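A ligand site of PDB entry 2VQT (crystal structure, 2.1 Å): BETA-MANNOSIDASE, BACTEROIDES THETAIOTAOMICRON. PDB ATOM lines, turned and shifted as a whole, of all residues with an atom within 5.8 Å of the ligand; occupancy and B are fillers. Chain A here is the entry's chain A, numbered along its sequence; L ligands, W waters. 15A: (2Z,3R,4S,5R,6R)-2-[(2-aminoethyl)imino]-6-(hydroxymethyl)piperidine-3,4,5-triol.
The side-chain hydroxyl (OH) of Tyr 512 sits at hydrogen-bond distance from an oxygen (O6) of the ligand (2.6 Å). The side-chain carboxylate (OD1) of Asp 174 sits at hydrogen-bond distance from an oxygen (O4) of the ligand. An oxygen (O2) of the ligand lies within hydrogen-bond range of the side-chain carboxylate (OE2) of Glu 530, at 2.7 Å. The side-chain carboxylate (OE1) of Glu 437 is in salt-bridge range of a nitrogen (N2) of the ligand (2.9 Å). The indole nitrogen (NE1) of Trp 175 lies within hydrogen-bond range of an oxygen (O4) of the ligand (2.9 Å). ND2 of Asn 436 lies within hydrogen-bond range of O2 of the ligand, 2.9 Å away. O3 of the ligand sits at hydrogen-bond distance from NE1 of Trp 173 (3.1 Å). A nitrogen (N1) of the ligand lies close to the indole nitrogen (NE1) of Trp 508 (3.3 Å). The indole nitrogen (NE1) of Trp 370 is in hydrogen-bond range of an oxygen (O2) of the ligand (3.4 Å).
The side-chain amide oxygen of Asn 153 sits at hydrogen-bond distance from the backbone NH of Asp 174. NE1 of Trp 508 sits at hydrogen-bond distance from OE1 of Glu 530 (2.9 Å). OE1 of Glu 530 sits close to ND1 of His 506 (3.3 Å). SG of Cys 399 is in hydrogen-bond range of OE1 of Glu 437, at 3.6 Å. The side-chain carboxylate of Glu 437 is in hydrogen-bond range of a ring nitrogen (ND1) of His 506, at 2.8 Å. The side-chain amide nitrogen (ND2) of Asn 436 sits close to the indole nitrogen (NE1) of Trp 370, 3.2 Å away. OD1 of Asn 436 lies within hydrogen-bond range of NH2 of Arg 368, at 3.0 Å. O of Trp 631 sits at hydrogen-bond distance from N of Gln 621 (3.1 Å).
Residues that only touch the ligand: Cys 399, Trp 445, Trp 620 and Trp 631. The nearest printed residue that does not touch the ligand is His 506 (4.5 Å).
Water W1 lies within hydrogen-bond range of O3 of the ligand (2.6 Å) and SG of Cys 399 (3.3 Å).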
ATOM      1  N   ASN A 153      20.550  22.856   1.786  1.00  0.00           N
ATOM      2  CA  ASN A 153      21.213  22.934   3.083  1.00  0.00           C
ATOM      3  C   ASN A 153      22.224  24.061   3.133  1.00  0.00           C
ATOM      4  O   ASN A 153      22.747  24.333   4.172  1.00  0.00           O
ATOM      5  CB  ASN A 153      21.849  21.602   3.437  1.00  0.00           C
ATOM      6  CG  ASN A 153      20.819  20.572   3.775  1.00  0.00           C
ATOM      7  OD1 ASN A 153      20.214  20.633   4.861  1.00  0.00           O
ATOM      8  ND2 ASN A 153      20.547  19.683   2.854  1.00  0.00           N
ATOM      9  N   TRP A 173      23.391  23.095   7.539  1.00  0.00           N
ATOM     10  CA  TRP A 173      22.799  21.782   7.292  1.00  0.00           C
ATOM     11  C   TRP A 173      21.552  21.657   8.147  1.00  0.00           C
ATOM     12  O   TRP A 173      21.289  22.536   8.950  1.00  0.00           O
ATOM     13  CB  TRP A 173      23.777  20.598   7.514  1.00  0.00           C
ATOM     14  CG  TRP A 173      23.436  19.464   6.504  1.00  0.00           C
ATOM     15  CD1 TRP A 173      22.626  18.373   6.729  1.00  0.00           C
ATOM     16  CD2 TRP A 173      23.904  19.342   5.151  1.00  0.00           C
ATOM     17  NE1 TRP A 173      22.511  17.601   5.577  1.00  0.00           N
ATOM     18  CE2 TRP A 173      23.276  18.205   4.586  1.00  0.00           C
ATOM     19  CE3 TRP A 173      24.789  20.107   4.351  1.00  0.00           C
ATOM     20  CZ2 TRP A 173      23.492  17.803   3.250  1.00  0.00           C
ATOM     21  CZ3 TRP A 173      24.992  19.720   3.024  1.00  0.00           C
ATOM     22  CH2 TRP A 173      24.341  18.570   2.487  1.00  0.00           C
ATOM     23  N   ASP A 174      20.749  20.599   7.991  1.00  0.00           N
ATOM     24  CA  ASP A 174      19.473  20.553   8.741  1.00  0.00           C
ATOM     25  C   ASP A 174      19.641  20.177  10.244  1.00  0.00           C
ATOM     26  O   ASP A 174      18.661  20.115  10.953  1.00  0.00           O
ATOM     27  CB  ASP A 174      18.414  19.702   8.052  1.00  0.00           C
ATOM     28  CG  ASP A 174      18.898  18.278   7.785  1.00  0.00           C
ATOM     29  OD1 ASP A 174      19.963  17.872   8.341  1.00  0.00           O
ATOM     30  OD2 ASP A 174      18.227  17.556   7.025  1.00  0.00           O
ATOM     31  N   TRP A 175      20.882  20.078  10.716  1.00  0.00           N
ATOM     32  CA  TRP A 175      21.215  19.990  12.158  1.00  0.00           C
ATOM     33  C   TRP A 175      22.347  20.953  12.486  1.00  0.00           C
ATOM     34  O   TRP A 175      22.977  20.874  13.548  1.00  0.00           O
ATOM     35  CB  TRP A 175      21.704  18.545  12.527  1.00  0.00           C
ATOM     36  CG  TRP A 175      22.512  17.884  11.374  1.00  0.00           C
ATOM     37  CD1 TRP A 175      22.082  16.904  10.521  1.00  0.00           C
ATOM     38  CD2 TRP A 175      23.870  18.186  10.968  1.00  0.00           C
ATOM     39  NE1 TRP A 175      23.076  16.575   9.609  1.00  0.00           N
ATOM     40  CE2 TRP A 175      24.191  17.322   9.881  1.00  0.00           C
ATOM     41  CE3 TRP A 175      24.869  19.078  11.452  1.00  0.00           C
ATOM     42  CZ2 TRP A 175      25.423  17.365   9.226  1.00  0.00           C
ATOM     43  CZ3 TRP A 175      26.114  19.121  10.784  1.00  0.00           C
ATOM     44  CH2 TRP A 175      26.378  18.239   9.684  1.00  0.00           C
ATOM     45  N   ARG A 368      29.630   5.177   9.065  1.00  0.00           N
ATOM     46  CA  ARG A 368      29.661   5.913   7.822  1.00  0.00           C
ATOM     47  C   ARG A 368      30.068   7.412   8.001  1.00  0.00           C
ATOM     48  O   ARG A 368      29.355   8.193   8.700  1.00  0.00           O
ATOM     49  CB  ARG A 368      28.334   5.812   7.120  1.00  0.00           C
ATOM     50  CG  ARG A 368      28.276   6.662   5.858  1.00  0.00           C
ATOM     51  CD  ARG A 368      27.012   6.293   5.029  1.00  0.00           C
ATOM     52  NE  ARG A 368      26.855   7.202   3.893  1.00  0.00           N
ATOM     53  CZ  ARG A 368      25.765   7.934   3.629  1.00  0.00           C
ATOM     54  NH1 ARG A 368      24.694   7.858   4.412  1.00  0.00           N
ATOM     55  NH2 ARG A 368      25.766   8.763   2.562  1.00  0.00           N
ATOM     56  N   TRP A 370      29.720  10.433   6.411  1.00  0.00           N
ATOM     57  CA  TRP A 370      28.762  10.957   5.462  1.00  0.00           C
ATOM     58  C   TRP A 370      29.325  12.170   4.668  1.00  0.00           C
ATOM     59  O   TRP A 370      30.141  12.975   5.172  1.00  0.00           O
ATOM     60  CB  TRP A 370      27.456  11.246   6.242  1.00  0.00           C
ATOM     61  CG  TRP A 370      26.531  12.222   5.677  1.00  0.00           C
ATOM     62  CD1 TRP A 370      25.423  11.931   4.956  1.00  0.00           C
ATOM     63  CD2 TRP A 370      26.539  13.639   5.875  1.00  0.00           C
ATOM     64  NE1 TRP A 370      24.760  13.109   4.614  1.00  0.00           N
ATOM     65  CE2 TRP A 370      25.444  14.166   5.171  1.00  0.00           C
ATOM     66  CE3 TRP A 370      27.403  14.528   6.525  1.00  0.00           C
ATOM     67  CZ2 TRP A 370      25.178  15.534   5.120  1.00  0.00           C
ATOM     68  CZ3 TRP A 370      27.129  15.880   6.475  1.00  0.00           C
ATOM     69  CH2 TRP A 370      26.028  16.367   5.792  1.00  0.00           C
ATOM     70  N   CYS A 399      23.698  15.654  -1.564  1.00  0.00           N
ATOM     71  CA  CYS A 399      22.345  16.193  -1.762  1.00  0.00           C
ATOM     72  C   CYS A 399      22.098  17.050  -2.999  1.00  0.00           C
ATOM     73  O   CYS A 399      20.958  17.152  -3.454  1.00  0.00           O
ATOM     74  CB  CYS A 399      21.809  16.860  -0.513  1.00  0.00           C
ATOM     75  SG  CYS A 399      21.617  15.709   0.849  1.00  0.00           S
ATOM     76  N   ASN A 436      26.342  11.392  -1.104  1.00  0.00           N
ATOM     77  CA  ASN A 436      25.093  11.160  -0.399  1.00  0.00           C
ATOM     78  C   ASN A 436      23.943  11.646  -1.244  1.00  0.00           C
ATOM     79  O   ASN A 436      23.777  12.873  -1.393  1.00  0.00           O
ATOM     80  CB  ASN A 436      25.088  11.936   0.950  1.00  0.00           C
ATOM     81  CG  ASN A 436      23.785  11.741   1.705  1.00  0.00           C
ATOM     82  OD1 ASN A 436      23.443  10.613   2.073  1.00  0.00           O
ATOM     83  ND2 ASN A 436      23.065  12.824   1.956  1.00  0.00           N
ATOM     84  N   GLU A 437      23.125  10.732  -1.752  1.00  0.00           N
ATOM     85  CA  GLU A 437      21.782  11.101  -2.254  1.00  0.00           C
ATOM     86  C   GLU A 437      21.683  11.952  -3.516  1.00  0.00           C
ATOM     87  O   GLU A 437      20.627  12.457  -3.818  1.00  0.00           O
ATOM     88  CB  GLU A 437      20.901  11.756  -1.157  1.00  0.00           C
ATOM     89  CG  GLU A 437      20.510  10.795  -0.069  1.00  0.00           C
ATOM     90  CD  GLU A 437      19.739  11.470   1.095  1.00  0.00           C
ATOM     91  OE1 GLU A 437      19.594  12.726   1.126  1.00  0.00           O
ATOM     92  OE2 GLU A 437      19.272  10.720   1.963  1.00  0.00           O
ATOM     93  N   TRP A 445      13.713  14.704  -6.711  1.00  0.00           N
ATOM     94  CA  TRP A 445      13.409  15.877  -5.896  1.00  0.00           C
ATOM     95  C   TRP A 445      12.858  17.034  -6.716  1.00  0.00           C
ATOM     96  O   TRP A 445      12.939  18.192  -6.284  1.00  0.00           O
ATOM     97  CB  TRP A 445      14.590  16.312  -4.996  1.00  0.00           C
ATOM     98  CG  TRP A 445      15.039  15.291  -3.982  1.00  0.00           C
ATOM     99  CD1 TRP A 445      14.448  14.050  -3.675  1.00  0.00           C
ATOM    100  CD2 TRP A 445      16.174  15.418  -3.107  1.00  0.00           C
ATOM    101  NE1 TRP A 445      15.194  13.410  -2.678  1.00  0.00           N
ATOM    102  CE2 TRP A 445      16.245  14.221  -2.325  1.00  0.00           C
ATOM    103  CE3 TRP A 445      17.156  16.414  -2.918  1.00  0.00           C
ATOM    104  CZ2 TRP A 445      17.262  14.005  -1.364  1.00  0.00           C
ATOM    105  CZ3 TRP A 445      18.177  16.188  -1.977  1.00  0.00           C
ATOM    106  CH2 TRP A 445      18.208  15.004  -1.211  1.00  0.00           C
ATOM    107  N   HIS A 506      17.982   4.479   2.270  1.00  0.00           N
ATOM    108  CA  HIS A 506      17.768   5.585   3.249  1.00  0.00           C
ATOM    109  C   HIS A 506      16.272   5.661   3.529  1.00  0.00           C
ATOM    110  O   HIS A 506      15.513   6.247   2.764  1.00  0.00           O
ATOM    111  CB  HIS A 506      18.261   6.942   2.703  1.00  0.00           C
ATOM    112  CG  HIS A 506      19.750   7.002   2.458  1.00  0.00           C
ATOM    113  ND1 HIS A 506      20.441   8.185   2.308  1.00  0.00           N
ATOM    114  CD2 HIS A 506      20.666   6.021   2.369  1.00  0.00           C
ATOM    115  CE1 HIS A 506      21.721   7.932   2.106  1.00  0.00           C
ATOM    116  NE2 HIS A 506      21.889   6.618   2.132  1.00  0.00           N
ATOM    117  N   TRP A 508      13.468   7.159   4.830  1.00  0.00           N
ATOM    118  CA  TRP A 508      12.996   8.318   5.546  1.00  0.00           C
ATOM    119  C   TRP A 508      11.483   8.355   5.627  1.00  0.00           C
ATOM    120  O   TRP A 508      10.875   9.398   5.852  1.00  0.00           O
ATOM    121  CB  TRP A 508      13.659   9.594   5.056  1.00  0.00           C
ATOM    122  CG  TRP A 508      15.069   9.643   5.526  1.00  0.00           C
ATOM    123  CD1 TRP A 508      16.191   9.290   4.820  1.00  0.00           C
ATOM    124  CD2 TRP A 508      15.518  10.010   6.828  1.00  0.00           C
ATOM    125  NE1 TRP A 508      17.326   9.435   5.598  1.00  0.00           N
ATOM    126  CE2 TRP A 508      16.941   9.883   6.841  1.00  0.00           C
ATOM    127  CE3 TRP A 508      14.853  10.419   8.001  1.00  0.00           C
ATOM    128  CZ2 TRP A 508      17.719  10.214   7.965  1.00  0.00           C
ATOM    129  CZ3 TRP A 508      15.623  10.724   9.142  1.00  0.00           C
ATOM    130  CH2 TRP A 508      17.046  10.620   9.123  1.00  0.00           C
ATOM    131  N   TRP A 511       9.995   9.552  10.288  1.00  0.00           N
ATOM    132  CA  TRP A 511      10.365  10.982  10.233  1.00  0.00           C
ATOM    133  C   TRP A 511       9.652  11.662   9.032  1.00  0.00           C
ATOM    134  O   TRP A 511       8.512  12.018   9.212  1.00  0.00           O
ATOM    135  CB  TRP A 511      11.889  11.270  10.335  1.00  0.00           C
ATOM    136  CG  TRP A 511      12.154  12.786  10.560  1.00  0.00           C
ATOM    137  CD1 TRP A 511      12.572  13.693   9.631  1.00  0.00           C
ATOM    138  CD2 TRP A 511      11.938  13.523  11.779  1.00  0.00           C
ATOM    139  NE1 TRP A 511      12.654  14.958  10.213  1.00  0.00           N
ATOM    140  CE2 TRP A 511      12.237  14.876  11.521  1.00  0.00           C
ATOM    141  CE3 TRP A 511      11.467  13.181  13.060  1.00  0.00           C
ATOM    142  CZ2 TRP A 511      12.125  15.873  12.498  1.00  0.00           C
ATOM    143  CZ3 TRP A 511      11.335  14.186  14.018  1.00  0.00           C
ATOM    144  CH2 TRP A 511      11.664  15.509  13.726  1.00  0.00           C
ATOM    145  N   TYR A 512      10.316  11.857   7.872  1.00  0.00           N
ATOM    146  CA  TYR A 512       9.716  12.643   6.761  1.00  0.00           C
ATOM    147  C   TYR A 512       8.417  12.088   6.253  1.00  0.00           C
ATOM    148  O   TYR A 512       7.513  12.857   6.008  1.00  0.00           O
ATOM    149  CB  TYR A 512      10.648  12.874   5.546  1.00  0.00           C
ATOM    150  CG  TYR A 512      11.850  13.699   5.901  1.00  0.00           C
ATOM    151  CD1 TYR A 512      11.758  15.092   5.969  1.00  0.00           C
ATOM    152  CD2 TYR A 512      13.078  13.089   6.205  1.00  0.00           C
ATOM    153  CE1 TYR A 512      12.894  15.869   6.350  1.00  0.00           C
ATOM    154  CE2 TYR A 512      14.208  13.854   6.564  1.00  0.00           C
ATOM    155  CZ  TYR A 512      14.097  15.238   6.638  1.00  0.00           C
ATOM    156  OH  TYR A 512      15.193  15.997   7.029  1.00  0.00           O
ATOM    157  N   GLU A 530      20.679   4.548   6.132  1.00  0.00           N
ATOM    158  CA  GLU A 530      20.204   5.679   6.976  1.00  0.00           C
ATOM    159  C   GLU A 530      18.781   5.403   7.375  1.00  0.00           C
ATOM    160  O   GLU A 530      18.029   4.958   6.564  1.00  0.00           O
ATOM    161  CB  GLU A 530      20.143   7.029   6.229  1.00  0.00           C
ATOM    162  CG  GLU A 530      21.470   7.581   5.741  1.00  0.00           C
ATOM    163  CD  GLU A 530      21.335   9.032   5.249  1.00  0.00           C
ATOM    164  OE1 GLU A 530      20.210   9.562   5.258  1.00  0.00           O
ATOM    165  OE2 GLU A 530      22.352   9.638   4.867  1.00  0.00           O
ATOM    166  N   TRP A 620      20.774   7.184  11.348  1.00  0.00           N
ATOM    167  CA  TRP A 620      21.008   8.602  11.257  1.00  0.00           C
ATOM    168  C   TRP A 620      20.513   9.260  12.586  1.00  0.00           C
ATOM    169  O   TRP A 620      19.325   9.278  12.782  1.00  0.00           O
ATOM    170  CB  TRP A 620      20.323   9.184   9.975  1.00  0.00           C
ATOM    171  CG  TRP A 620      20.786  10.594   9.859  1.00  0.00           C
ATOM    172  CD1 TRP A 620      20.310  11.688  10.541  1.00  0.00           C
ATOM    173  CD2 TRP A 620      21.979  11.036   9.155  1.00  0.00           C
ATOM    174  NE1 TRP A 620      21.113  12.799  10.268  1.00  0.00           N
ATOM    175  CE2 TRP A 620      22.137  12.415   9.428  1.00  0.00           C
ATOM    176  CE3 TRP A 620      22.890  10.404   8.320  1.00  0.00           C
ATOM    177  CZ2 TRP A 620      23.213  13.160   8.888  1.00  0.00           C
ATOM    178  CZ3 TRP A 620      23.942  11.129   7.765  1.00  0.00           C
ATOM    179  CH2 TRP A 620      24.097  12.504   8.060  1.00  0.00           C
ATOM    180  N   GLN A 621      21.377   9.841  13.460  1.00  0.00           N
ATOM    181  CA  GLN A 621      22.833  10.016  13.235  1.00  0.00           C
ATOM    182  C   GLN A 621      23.517   9.756  14.574  1.00  0.00           C
ATOM    183  O   GLN A 621      22.842   9.739  15.603  1.00  0.00           O
ATOM    184  CB  GLN A 621      23.180  11.440  12.770  1.00  0.00           C
ATOM    185  CG  GLN A 621      22.895  12.560  13.880  1.00  0.00           C
ATOM    186  CD  GLN A 621      22.673  13.978  13.313  1.00  0.00           C
ATOM    187  OE1 GLN A 621      21.630  14.239  12.776  1.00  0.00           O
ATOM    188  NE2 GLN A 621      23.667  14.887  13.452  1.00  0.00           N
ATOM    189  N   TRP A 631      18.828  14.314  15.188  1.00  0.00           N
ATOM    190  CA  TRP A 631      18.626  12.895  15.132  1.00  0.00           C
ATOM    191  C   TRP A 631      19.731  12.146  15.887  1.00  0.00           C
ATOM    192  O   TRP A 631      19.775  10.924  15.878  1.00  0.00           O
ATOM    193  CB  TRP A 631      18.687  12.503  13.651  1.00  0.00           C
ATOM    194  CG  TRP A 631      17.601  13.187  12.765  1.00  0.00           C
ATOM    195  CD1 TRP A 631      16.442  12.662  12.391  1.00  0.00           C
ATOM    196  CD2 TRP A 631      17.677  14.499  12.178  1.00  0.00           C
ATOM    197  NE1 TRP A 631      15.759  13.563  11.582  1.00  0.00           N
ATOM    198  CE2 TRP A 631      16.529  14.700  11.437  1.00  0.00           C
ATOM    199  CE3 TRP A 631      18.681  15.527  12.170  1.00  0.00           C
ATOM    200  CZ2 TRP A 631      16.272  15.917  10.714  1.00  0.00           C
ATOM    201  CZ3 TRP A 631      18.424  16.733  11.463  1.00  0.00           C
ATOM    202  CH2 TRP A 631      17.224  16.899  10.770  1.00  0.00           C
HETATM  203  O6  15A L   1      17.457  14.927   7.580  1.00  0.00           O
HETATM  204  C6  15A L   1      18.398  14.492   8.396  1.00  0.00           C
HETATM  205  C5  15A L   1      19.518  13.863   7.530  1.00  0.00           C
HETATM  206  C4  15A L   1      20.490  14.842   6.799  1.00  0.00           C
HETATM  207  O4  15A L   1      21.177  15.586   7.711  1.00  0.00           O
HETATM  208  C3  15A L   1      21.443  14.136   5.764  1.00  0.00           C
HETATM  209  O3  15A L   1      21.606  14.827   4.652  1.00  0.00           O
HETATM  210  C2  15A L   1      20.981  12.684   5.409  1.00  0.00           C
HETATM  211  O2  15A L   1      21.531  12.135   4.282  1.00  0.00           O
HETATM  212  N5  15A L   1      18.907  12.988   6.600  1.00  0.00           N
HETATM  213  C1  15A L   1      19.466  12.595   5.436  1.00  0.00           C
HETATM  214  N1  15A L   1      18.772  12.136   4.383  1.00  0.00           N
HETATM  215  C7  15A L   1      17.368  12.264   4.162  1.00  0.00           C
HETATM  216  C8  15A L   1      16.835  13.644   3.672  1.00  0.00           C
HETATM  217  N2  15A L   1      17.240  13.875   2.274  1.00  0.00           N
HETATM  218  O   HOH W   1      19.454  15.583   3.327  1.00  0.00           O
